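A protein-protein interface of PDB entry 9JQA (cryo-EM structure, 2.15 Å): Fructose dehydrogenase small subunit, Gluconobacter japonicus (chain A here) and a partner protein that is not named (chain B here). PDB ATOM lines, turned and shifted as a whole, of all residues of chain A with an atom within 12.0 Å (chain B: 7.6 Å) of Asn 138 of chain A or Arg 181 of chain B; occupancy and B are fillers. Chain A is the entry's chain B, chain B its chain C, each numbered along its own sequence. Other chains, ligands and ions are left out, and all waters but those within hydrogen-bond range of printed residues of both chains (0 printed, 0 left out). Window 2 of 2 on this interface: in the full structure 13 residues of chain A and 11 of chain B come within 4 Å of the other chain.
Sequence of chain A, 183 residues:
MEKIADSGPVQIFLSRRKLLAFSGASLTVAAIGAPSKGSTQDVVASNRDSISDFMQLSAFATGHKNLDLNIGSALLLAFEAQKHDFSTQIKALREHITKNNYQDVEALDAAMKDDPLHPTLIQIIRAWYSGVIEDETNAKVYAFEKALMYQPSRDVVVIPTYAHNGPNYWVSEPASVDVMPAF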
ATOM      1  N   ALA A  78      -2.413 -28.867  18.132  1.00  0.00           N
ATOM      2  CA  ALA A  78      -3.296 -27.709  18.075  1.00  0.00           C
ATOM      3  C   ALA A  78      -3.100 -26.920  16.785  1.00  0.00           C
ATOM      4  O   ALA A  78      -4.072 -26.471  16.169  1.00  0.00           O
ATOM      5  CB  ALA A  78      -3.065 -26.819  19.290  1.00  0.00           C
ATOM      6  N   GLN A  82      -5.801 -26.140  13.857  1.00  0.00           N
ATOM      7  CA  GLN A  82      -6.111 -24.785  13.413  1.00  0.00           C
ATOM      8  C   GLN A  82      -5.862 -24.614  11.922  1.00  0.00           C
ATOM      9  O   GLN A  82      -6.700 -24.057  11.203  1.00  0.00           O
ATOM     10  CB  GLN A  82      -5.275 -23.783  14.207  1.00  0.00           C
ATOM     11  CG  GLN A  82      -5.907 -22.422  14.388  1.00  0.00           C
ATOM     12  CD  GLN A  82      -5.000 -21.473  15.141  1.00  0.00           C
ATOM     13  OE1 GLN A  82      -3.793 -21.443  14.913  1.00  0.00           O
ATOM     14  NE2 GLN A  82      -5.577 -20.696  16.048  1.00  0.00           N
ATOM     15  N   SER A 130       4.203 -17.690  25.041  1.00  0.00           N
ATOM     16  CA  SER A 130       3.030 -17.397  25.851  1.00  0.00           C
ATOM     17  C   SER A 130       2.265 -18.639  26.278  1.00  0.00           C
ATOM     18  O   SER A 130       1.484 -18.569  27.232  1.00  0.00           O
ATOM     19  CB  SER A 130       2.084 -16.469  25.086  1.00  0.00           C
ATOM     20  OG  SER A 130       1.636 -17.080  23.893  1.00  0.00           O
ATOM     21  N   GLY A 131       2.467 -19.767  25.605  1.00  0.00           N
ATOM     22  CA  GLY A 131       1.745 -20.975  25.925  1.00  0.00           C
ATOM     23  C   GLY A 131       0.368 -21.085  25.313  1.00  0.00           C
ATOM     24  O   GLY A 131      -0.339 -22.057  25.600  1.00  0.00           O
ATOM     25  N   VAL A 132      -0.041 -20.125  24.484  1.00  0.00           N
ATOM     26  CA  VAL A 132      -1.340 -20.154  23.831  1.00  0.00           C
ATOM     27  C   VAL A 132      -1.146 -19.935  22.339  1.00  0.00           C
ATOM     28  O   VAL A 132      -0.146 -19.372  21.891  1.00  0.00           O
ATOM     29  CB  VAL A 132      -2.316 -19.100  24.393  1.00  0.00           C
ATOM     30  CG1 VAL A 132      -2.793 -19.500  25.768  1.00  0.00           C
ATOM     31  CG2 VAL A 132      -1.664 -17.735  24.421  1.00  0.00           C
ATOM     32  N   ILE A 133      -2.133 -20.385  21.572  1.00  0.00           N
ATOM     33  CA  ILE A 133      -2.142 -20.228  20.129  1.00  0.00           C
ATOM     34  C   ILE A 133      -3.187 -19.214  19.681  1.00  0.00           C
ATOM     35  O   ILE A 133      -2.934 -18.419  18.774  1.00  0.00           O
ATOM     36  CB  ILE A 133      -2.360 -21.594  19.444  1.00  0.00           C
ATOM     37  CG1 ILE A 133      -1.132 -22.477  19.654  1.00  0.00           C
ATOM     38  CG2 ILE A 133      -2.642 -21.421  17.969  1.00  0.00           C
ATOM     39  CD1 ILE A 133      -1.209 -23.797  18.954  1.00  0.00           C
ATOM     40  N   GLU A 134      -4.353 -19.215  20.313  1.00  0.00           N
ATOM     41  CA  GLU A 134      -5.391 -18.244  20.017  1.00  0.00           C
ATOM     42  C   GLU A 134      -5.299 -17.060  20.976  1.00  0.00           C
ATOM     43  O   GLU A 134      -4.588 -17.091  21.980  1.00  0.00           O
ATOM     44  CB  GLU A 134      -6.770 -18.895  20.099  1.00  0.00           C
ATOM     45  CG  GLU A 134      -7.255 -19.466  18.783  1.00  0.00           C
ATOM     46  CD  GLU A 134      -7.727 -20.896  18.912  1.00  0.00           C
ATOM     47  OE1 GLU A 134      -8.344 -21.226  19.945  1.00  0.00           O
ATOM     48  OE2 GLU A 134      -7.479 -21.691  17.982  1.00  0.00           O
ATOM     49  N   ASP A 135      -6.041 -16.003  20.655  1.00  0.00           N
ATOM     50  CA  ASP A 135      -6.013 -14.755  21.409  1.00  0.00           C
ATOM     51  C   ASP A 135      -7.346 -14.478  22.095  1.00  0.00           C
ATOM     52  O   ASP A 135      -7.801 -13.335  22.161  1.00  0.00           O
ATOM     53  CB  ASP A 135      -5.634 -13.589  20.502  1.00  0.00           C
ATOM     54  CG  ASP A 135      -6.288 -13.679  19.138  1.00  0.00           C
ATOM     55  OD1 ASP A 135      -6.364 -14.799  18.588  1.00  0.00           O
ATOM     56  OD2 ASP A 135      -6.727 -12.633  18.616  1.00  0.00           O
ATOM     57  N   GLU A 136      -7.985 -15.517  22.619  1.00  0.00           N
ATOM     58  CA  GLU A 136      -9.262 -15.397  23.304  1.00  0.00           C
ATOM     59  C   GLU A 136      -9.082 -15.673  24.794  1.00  0.00           C
ATOM     60  O   GLU A 136      -7.978 -15.929  25.279  1.00  0.00           O
ATOM     61  CB  GLU A 136     -10.291 -16.349  22.693  1.00  0.00           C
ATOM     62  CG  GLU A 136     -10.303 -16.361  21.177  1.00  0.00           C
ATOM     63  CD  GLU A 136     -10.446 -17.759  20.611  1.00  0.00           C
ATOM     64  OE1 GLU A 136      -9.956 -18.713  21.249  1.00  0.00           O
ATOM     65  OE2 GLU A 136     -11.054 -17.904  19.529  1.00  0.00           O
ATOM     66  N   THR A 137     -10.196 -15.608  25.522  1.00  0.00           N
ATOM     67  CA  THR A 137     -10.221 -15.951  26.937  1.00  0.00           C
ATOM     68  C   THR A 137     -10.376 -17.449  27.162  1.00  0.00           C
ATOM     69  O   THR A 137      -9.884 -17.978  28.165  1.00  0.00           O
ATOM     70  CB  THR A 137     -11.360 -15.192  27.633  1.00  0.00           C
ATOM     71  OG1 THR A 137     -11.117 -13.783  27.545  1.00  0.00           O
ATOM     72  CG2 THR A 137     -11.479 -15.587  29.097  1.00  0.00           C
ATOM     73  N   ASN A 138     -11.027 -18.146  26.237  1.00  0.00           N
ATOM     74  CA  ASN A 138     -11.197 -19.587  26.317  1.00  0.00           C
ATOM     75  C   ASN A 138     -10.067 -20.348  25.638  1.00  0.00           C
ATOM     76  O   ASN A 138     -10.146 -21.575  25.521  1.00  0.00           O
ATOM     77  CB  ASN A 138     -12.535 -19.992  25.699  1.00  0.00           C
ATOM     78  CG  ASN A 138     -12.681 -19.511  24.271  1.00  0.00           C
ATOM     79  OD1 ASN A 138     -12.646 -18.310  24.002  1.00  0.00           O
ATOM     80  ND2 ASN A 138     -12.841 -20.447  23.344  1.00  0.00           N
ATOM     81  N   ALA A 139      -9.033 -19.649  25.175  1.00  0.00           N
ATOM     82  CA  ALA A 139      -7.929 -20.305  24.491  1.00  0.00           C
ATOM     83  C   ALA A 139      -7.244 -21.304  25.413  1.00  0.00           C
ATOM     84  O   ALA A 139      -7.061 -21.051  26.607  1.00  0.00           O
ATOM     85  CB  ALA A 139      -6.920 -19.269  23.998  1.00  0.00           C
ATOM     86  N   LYS A 140      -6.871 -22.448  24.851  1.00  0.00           N
ATOM     87  CA  LYS A 140      -6.204 -23.481  25.628  1.00  0.00           C
ATOM     88  C   LYS A 140      -4.774 -23.062  25.938  1.00  0.00           C
ATOM     89  O   LYS A 140      -4.042 -22.610  25.054  1.00  0.00           O
ATOM     90  CB  LYS A 140      -6.216 -24.805  24.868  1.00  0.00           C
ATOM     91  CG  LYS A 140      -7.597 -25.258  24.435  1.00  0.00           C
ATOM     92  CD  LYS A 140      -7.640 -26.745  24.107  1.00  0.00           C
ATOM     93  CE  LYS A 140      -6.607 -27.536  24.895  1.00  0.00           C
ATOM     94  NZ  LYS A 140      -6.270 -28.831  24.243  1.00  0.00           N
ATOM     95  N   VAL A 141      -4.379 -23.208  27.196  1.00  0.00           N
ATOM     96  CA  VAL A 141      -3.010 -22.943  27.615  1.00  0.00           C
ATOM     97  C   VAL A 141      -2.238 -24.250  27.547  1.00  0.00           C
ATOM     98  O   VAL A 141      -2.566 -25.214  28.246  1.00  0.00           O
ATOM     99  CB  VAL A 141      -2.962 -22.344  29.027  1.00  0.00           C
ATOM    100  CG1 VAL A 141      -1.557 -22.426  29.590  1.00  0.00           C
ATOM    101  CG2 VAL A 141      -3.431 -20.910  29.001  1.00  0.00           C
ATOM    102  N   TYR A 142      -1.224 -24.292  26.693  1.00  0.00           N
ATOM    103  CA  TYR A 142      -0.400 -25.481  26.553  1.00  0.00           C
ATOM    104  C   TYR A 142       0.857 -25.427  27.401  1.00  0.00           C
ATOM    105  O   TYR A 142       1.548 -26.443  27.518  1.00  0.00           O
ATOM    106  CB  TYR A 142      -0.035 -25.687  25.081  1.00  0.00           C
ATOM    107  CG  TYR A 142      -1.255 -25.782  24.205  1.00  0.00           C
ATOM    108  CD1 TYR A 142      -1.907 -26.990  24.027  1.00  0.00           C
ATOM    109  CD2 TYR A 142      -1.781 -24.657  23.590  1.00  0.00           C
ATOM    110  CE1 TYR A 142      -3.032 -27.081  23.244  1.00  0.00           C
ATOM    111  CE2 TYR A 142      -2.907 -24.739  22.805  1.00  0.00           C
ATOM    112  CZ  TYR A 142      -3.529 -25.954  22.636  1.00  0.00           C
ATOM    113  OH  TYR A 142      -4.654 -26.036  21.854  1.00  0.00           O
ATOM    114  N   ALA A 143       1.157 -24.281  28.005  1.00  0.00           N
ATOM    115  CA  ALA A 143       2.318 -24.166  28.873  1.00  0.00           C
ATOM    116  C   ALA A 143       2.214 -22.963  29.799  1.00  0.00           C
ATOM    117  O   ALA A 143       1.992 -21.833  29.355  1.00  0.00           O
ATOM    118  CB  ALA A 143       3.602 -24.085  28.047  1.00  0.00           C
ATOM    119  N   PHE A 144       2.352 -23.220  31.092  1.00  0.00           N
ATOM    120  CA  PHE A 144       2.617 -22.214  32.104  1.00  0.00           C
ATOM    121  C   PHE A 144       3.851 -22.681  32.861  1.00  0.00           C
ATOM    122  O   PHE A 144       4.093 -23.884  32.990  1.00  0.00           O
ATOM    123  CB  PHE A 144       1.418 -22.040  33.051  1.00  0.00           C
ATOM    124  CG  PHE A 144       1.578 -20.937  34.060  1.00  0.00           C
ATOM    125  CD1 PHE A 144       1.787 -19.629  33.660  1.00  0.00           C
ATOM    126  CD2 PHE A 144       1.499 -21.210  35.413  1.00  0.00           C
ATOM    127  CE1 PHE A 144       1.920 -18.622  34.592  1.00  0.00           C
ATOM    128  CE2 PHE A 144       1.635 -20.210  36.344  1.00  0.00           C
ATOM    129  CZ  PHE A 144       1.843 -18.914  35.935  1.00  0.00           C
ATOM    130  N   VAL B 174       0.008 -29.539  31.182  1.00  0.00           N
ATOM    131  CA  VAL B 174      -0.754 -28.300  31.293  1.00  0.00           C
ATOM    132  C   VAL B 174      -1.920 -28.310  30.314  1.00  0.00           C
ATOM    133  O   VAL B 174      -3.024 -27.859  30.638  1.00  0.00           O
ATOM    134  CB  VAL B 174       0.167 -27.088  31.072  1.00  0.00           C
ATOM    135  CG1 VAL B 174      -0.644 -25.822  30.882  1.00  0.00           C
ATOM    136  CG2 VAL B 174       1.118 -26.934  32.235  1.00  0.00           C
ATOM    137  N   ALA B 175      -1.698 -28.837  29.109  1.00  0.00           N
ATOM    138  CA  ALA B 175      -2.750 -28.857  28.100  1.00  0.00           C
ATOM    139  C   ALA B 175      -3.946 -29.679  28.559  1.00  0.00           C
ATOM    140  O   ALA B 175      -5.097 -29.261  28.390  1.00  0.00           O
ATOM    141  CB  ALA B 175      -2.199 -29.401  26.784  1.00  0.00           C
ATOM    142  N   ASN B 176      -3.693 -30.843  29.161  1.00  0.00           N
ATOM    143  CA  ASN B 176      -4.782 -31.712  29.588  1.00  0.00           C
ATOM    144  C   ASN B 176      -5.636 -31.083  30.678  1.00  0.00           C
ATOM    145  O   ASN B 176      -6.782 -31.503  30.871  1.00  0.00           O
ATOM    146  CB  ASN B 176      -4.223 -33.050  30.066  1.00  0.00           C
ATOM    147  CG  ASN B 176      -3.851 -33.963  28.920  1.00  0.00           C
ATOM    148  OD1 ASN B 176      -4.258 -33.743  27.781  1.00  0.00           O
ATOM    149  ND2 ASN B 176      -3.072 -34.995  29.214  1.00  0.00           N
ATOM    150  N   ALA B 177      -5.113 -30.090  31.391  1.00  0.00           N
ATOM    151  CA  ALA B 177      -5.898 -29.381  32.390  1.00  0.00           C
ATOM    152  C   ALA B 177      -6.910 -28.425  31.777  1.00  0.00           C
ATOM    153  O   ALA B 177      -7.822 -27.982  32.483  1.00  0.00           O
ATOM    154  CB  ALA B 177      -4.976 -28.610  33.335  1.00  0.00           C
ATOM    155  N   ASN B 178      -6.780 -28.104  30.486  1.00  0.00           N
ATOM    156  CA  ASN B 178      -7.681 -27.139  29.868  1.00  0.00           C
ATOM    157  C   ASN B 178      -9.121 -27.625  29.875  1.00  0.00           C
ATOM    158  O   ASN B 178     -10.048 -26.814  29.972  1.00  0.00           O
ATOM    159  CB  ASN B 178      -7.233 -26.842  28.440  1.00  0.00           C
ATOM    160  CG  ASN B 178      -6.012 -25.958  28.390  1.00  0.00           C
ATOM    161  OD1 ASN B 178      -5.992 -24.875  28.969  1.00  0.00           O
ATOM    162  ND2 ASN B 178      -4.979 -26.417  27.698  1.00  0.00           N
ATOM    163  N   SER B 179      -9.333 -28.937  29.766  1.00  0.00           N
ATOM    164  CA  SER B 179     -10.686 -29.472  29.830  1.00  0.00           C
ATOM    165  C   SER B 179     -11.292 -29.339  31.218  1.00  0.00           C
ATOM    166  O   SER B 179     -12.519 -29.372  31.350  1.00  0.00           O
ATOM    167  CB  SER B 179     -10.694 -30.937  29.399  1.00  0.00           C
ATOM    168  OG  SER B 179     -10.063 -31.754  30.366  1.00  0.00           O
ATOM    169  N   ARG B 180     -10.469 -29.189  32.251  1.00  0.00           N
ATOM    170  CA  ARG B 180     -10.964 -29.077  33.614  1.00  0.00           C
ATOM    171  C   ARG B 180     -11.232 -27.640  34.029  1.00  0.00           C
ATOM    172  O   ARG B 180     -11.636 -27.407  35.171  1.00  0.00           O
ATOM    173  CB  ARG B 180      -9.983 -29.726  34.590  1.00  0.00           C
ATOM    174  CG  ARG B 180      -9.952 -31.235  34.494  1.00  0.00           C
ATOM    175  CD  ARG B 180      -9.173 -31.835  35.637  1.00  0.00           C
ATOM    176  NE  ARG B 180      -7.781 -31.408  35.624  1.00  0.00           N
ATOM    177  CZ  ARG B 180      -6.834 -31.973  34.890  1.00  0.00           C
ATOM    178  NH1 ARG B 180      -7.094 -32.993  34.092  1.00  0.00           N
ATOM    179  NH2 ARG B 180      -5.594 -31.499  34.956  1.00  0.00           N
ATOM    180  N   ARG B 181     -11.014 -26.675  33.145  1.00  0.00           N
ATOM    181  CA  ARG B 181     -11.505 -25.335  33.407  1.00  0.00           C
ATOM    182  C   ARG B 181     -13.029 -25.350  33.377  1.00  0.00           C
ATOM    183  O   ARG B 181     -13.654 -26.283  32.866  1.00  0.00           O
ATOM    184  CB  ARG B 181     -10.949 -24.342  32.389  1.00  0.00           C
ATOM    185  CG  ARG B 181      -9.435 -24.241  32.404  1.00  0.00           C
ATOM    186  CD  ARG B 181      -8.923 -23.293  31.340  1.00  0.00           C
ATOM    187  NE  ARG B 181      -9.363 -23.678  30.007  1.00  0.00           N
ATOM    188  CZ  ARG B 181      -8.988 -23.072  28.890  1.00  0.00           C
ATOM    189  NH1 ARG B 181      -8.152 -22.047  28.907  1.00  0.00           N
ATOM    190  NH2 ARG B 181      -9.463 -23.504  27.726  1.00  0.00           N
ATOM    191  N   SER B 182     -13.625 -24.311  33.953  1.00  0.00           N
ATOM    192  CA  SER B 182     -15.062 -24.257  34.217  1.00  0.00           C
ATOM    193  C   SER B 182     -15.498 -25.322  35.217  1.00  0.00           C
ATOM    194  O   SER B 182     -16.685 -25.640  35.313  1.00  0.00           O
ATOM    195  CB  SER B 182     -15.886 -24.372  32.930  1.00  0.00           C
ATOM    196  OG  SER B 182     -16.098 -25.727  32.586  1.00  0.00           O
ATOM    197  N   ASN B 183     -14.552 -25.875  35.970  1.00  0.00           N
ATOM    198  CA  ASN B 183     -14.836 -26.727  37.115  1.00  0.00           C
ATOM    199  C   ASN B 183     -14.492 -25.960  38.381  1.00  0.00           C
ATOM    200  O   ASN B 183     -13.450 -25.300  38.444  1.00  0.00           O
ATOM    201  CB  ASN B 183     -14.033 -28.027  37.061  1.00  0.00           C
ATOM    202  CG  ASN B 183     -14.621 -29.039  36.110  1.00  0.00           C
ATOM    203  OD1 ASN B 183     -15.716 -28.852  35.582  1.00  0.00           O
ATOM    204  ND2 ASN B 183     -13.897 -30.125  35.885  1.00  0.00           N
ATOM    205  N   SER B 184     -15.367 -26.033  39.377  1.00  0.00           N
ATOM    206  CA  SER B 184     -15.142 -25.326  40.628  1.00  0.00           C
ATOM    207  C   SER B 184     -14.508 -26.194  41.706  1.00  0.00           C
ATOM    208  O   SER B 184     -14.039 -25.656  42.712  1.00  0.00           O
ATOM    209  CB  SER B 184     -16.459 -24.746  41.152  1.00  0.00           C
ATOM    210  OG  SER B 184     -17.230 -24.197  40.100  1.00  0.00           O
ATOM    211  N   LYS B 188     -13.444 -33.879  39.466  1.00  0.00           N
ATOM    212  CA  LYS B 188     -13.147 -34.453  38.164  1.00  0.00           C
ATOM    213  C   LYS B 188     -11.658 -34.451  37.845  1.00  0.00           C
ATOM    214  O   LYS B 188     -11.274 -34.840  36.739  1.00  0.00           O
ATOM    215  CB  LYS B 188     -13.921 -33.709  37.074  1.00  0.00           C
ATOM    216  CG  LYS B 188     -15.426 -33.858  37.202  1.00  0.00           C
ATOM    217  CD  LYS B 188     -16.142 -33.506  35.915  1.00  0.00           C
ATOM    218  CE  LYS B 188     -17.353 -32.631  36.184  1.00  0.00           C
ATOM    219  NZ  LYS B 188     -17.701 -31.784  35.012  1.00  0.00           N
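The guanidinium group of Arg 181 of chain B is in hydrogen-bond range of the backbone carbonyl oxygen of Asn 138 of chain A (3.0 Å). NH1 of Arg 181 of chain B is in hydrogen-bond range of O of Ala 139 of chain A (2.7 Å). The backbone carbonyl oxygen of Val 141 of chain A is in hydrogen-bond range of the side-chain amide nitrogen of Asn 178 of chain B (2.8 Å).
ND2 of Asn 178 of chain B sits at hydrogen-bond distance from O of Ala 175 of chain B (2.9 Å). N of Tyr 142 of chain A lies within hydrogen-bond range of O of Gly 131 of chain A. O of Asn 178 of chain B sits at hydrogen-bond distance from NE of Arg 181 of chain B (3.2 Å).
Among the printed residues, merely in contact across the chains: Lys 140 of chain A with Asn 178 of chain B (3.4 Å), Lys 140 of chain A with Arg 181 of chain B (3.9 Å), Val 141 of chain A with Val 174 of chain B (3.3 Å), Val 141 of chain A with Ala 175 of chain B (3.7 Å), Tyr 142 of chain A with Val 174 of chain B (3.8 Å), Tyr 142 of chain A with Ala 175 of chain B (3.7 Å), Ala 143 of chain A with Val 174 of chain B (3.7 Å) and Phe 144 of chain A with Val 174 of chain B (3.97 Å).
Of chain B, only Arg 181 (3.0 Å) comes within 4 Å of Asn 138 of chain A. Arg 181 of chain B touches just these residues of chain A: Asn 138, Ala 139 and Lys 140. No residue of chain A comes within 4 Å of Ala 177 of chain B. No residue of chain A comes within 4 Å of Arg 180 of chain B. No residue of chain A comes within 4 Å of Ser 182 of chain B. No residue of chain A comes within 4 Å of Asn 183 of chain B. Printed residues of chain B within 4 Å of Tyr 142 of chain A: Val 174 (3.8 Å) and Ala 175 (3.7 Å). Printed residues of chain B within 4 Å of Val 141 of chain A: Val 174 (3.3 Å), Ala 175 (3.7 Å) and Asn 178 (2.8 Å). Of the printed residues of chain B, Ala 143 of chain A touches Val 174 (3.7 Å). Printed residues of chain B within 4 Å of Phe 144 of chain A: Val 174 (3.97 Å). Of the printed residues of chain B, Lys 140 of chain A touches Asn 178 and Arg 181. Val 132 of chain A touches none of the printed residues of chain B. Asp 135 of chain A touches none of the printed residues of chain B. The nearest printed residue of chain B that does not touch Lys 140 of chain A is Ala 175 of chain B (4.2 Å).
Printed residues of chain B that touch a printed residue of chain A: Val 174, Ala 175, Asn 178 and Arg 181. Hydrophobic or aromatic side chains of chain B within 4 Å of the printed part of chain A: Val 174 and Ala 175. Along chain B the printed residues that touch a printed residue of chain A span positions 174 to 181. Among the printed residues, 11 pairs touch across the chains. Among the printed residues, no Asp or Glu carboxylate lies within 4 Å of a Lys or Arg side-chain nitrogen of the other chain.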
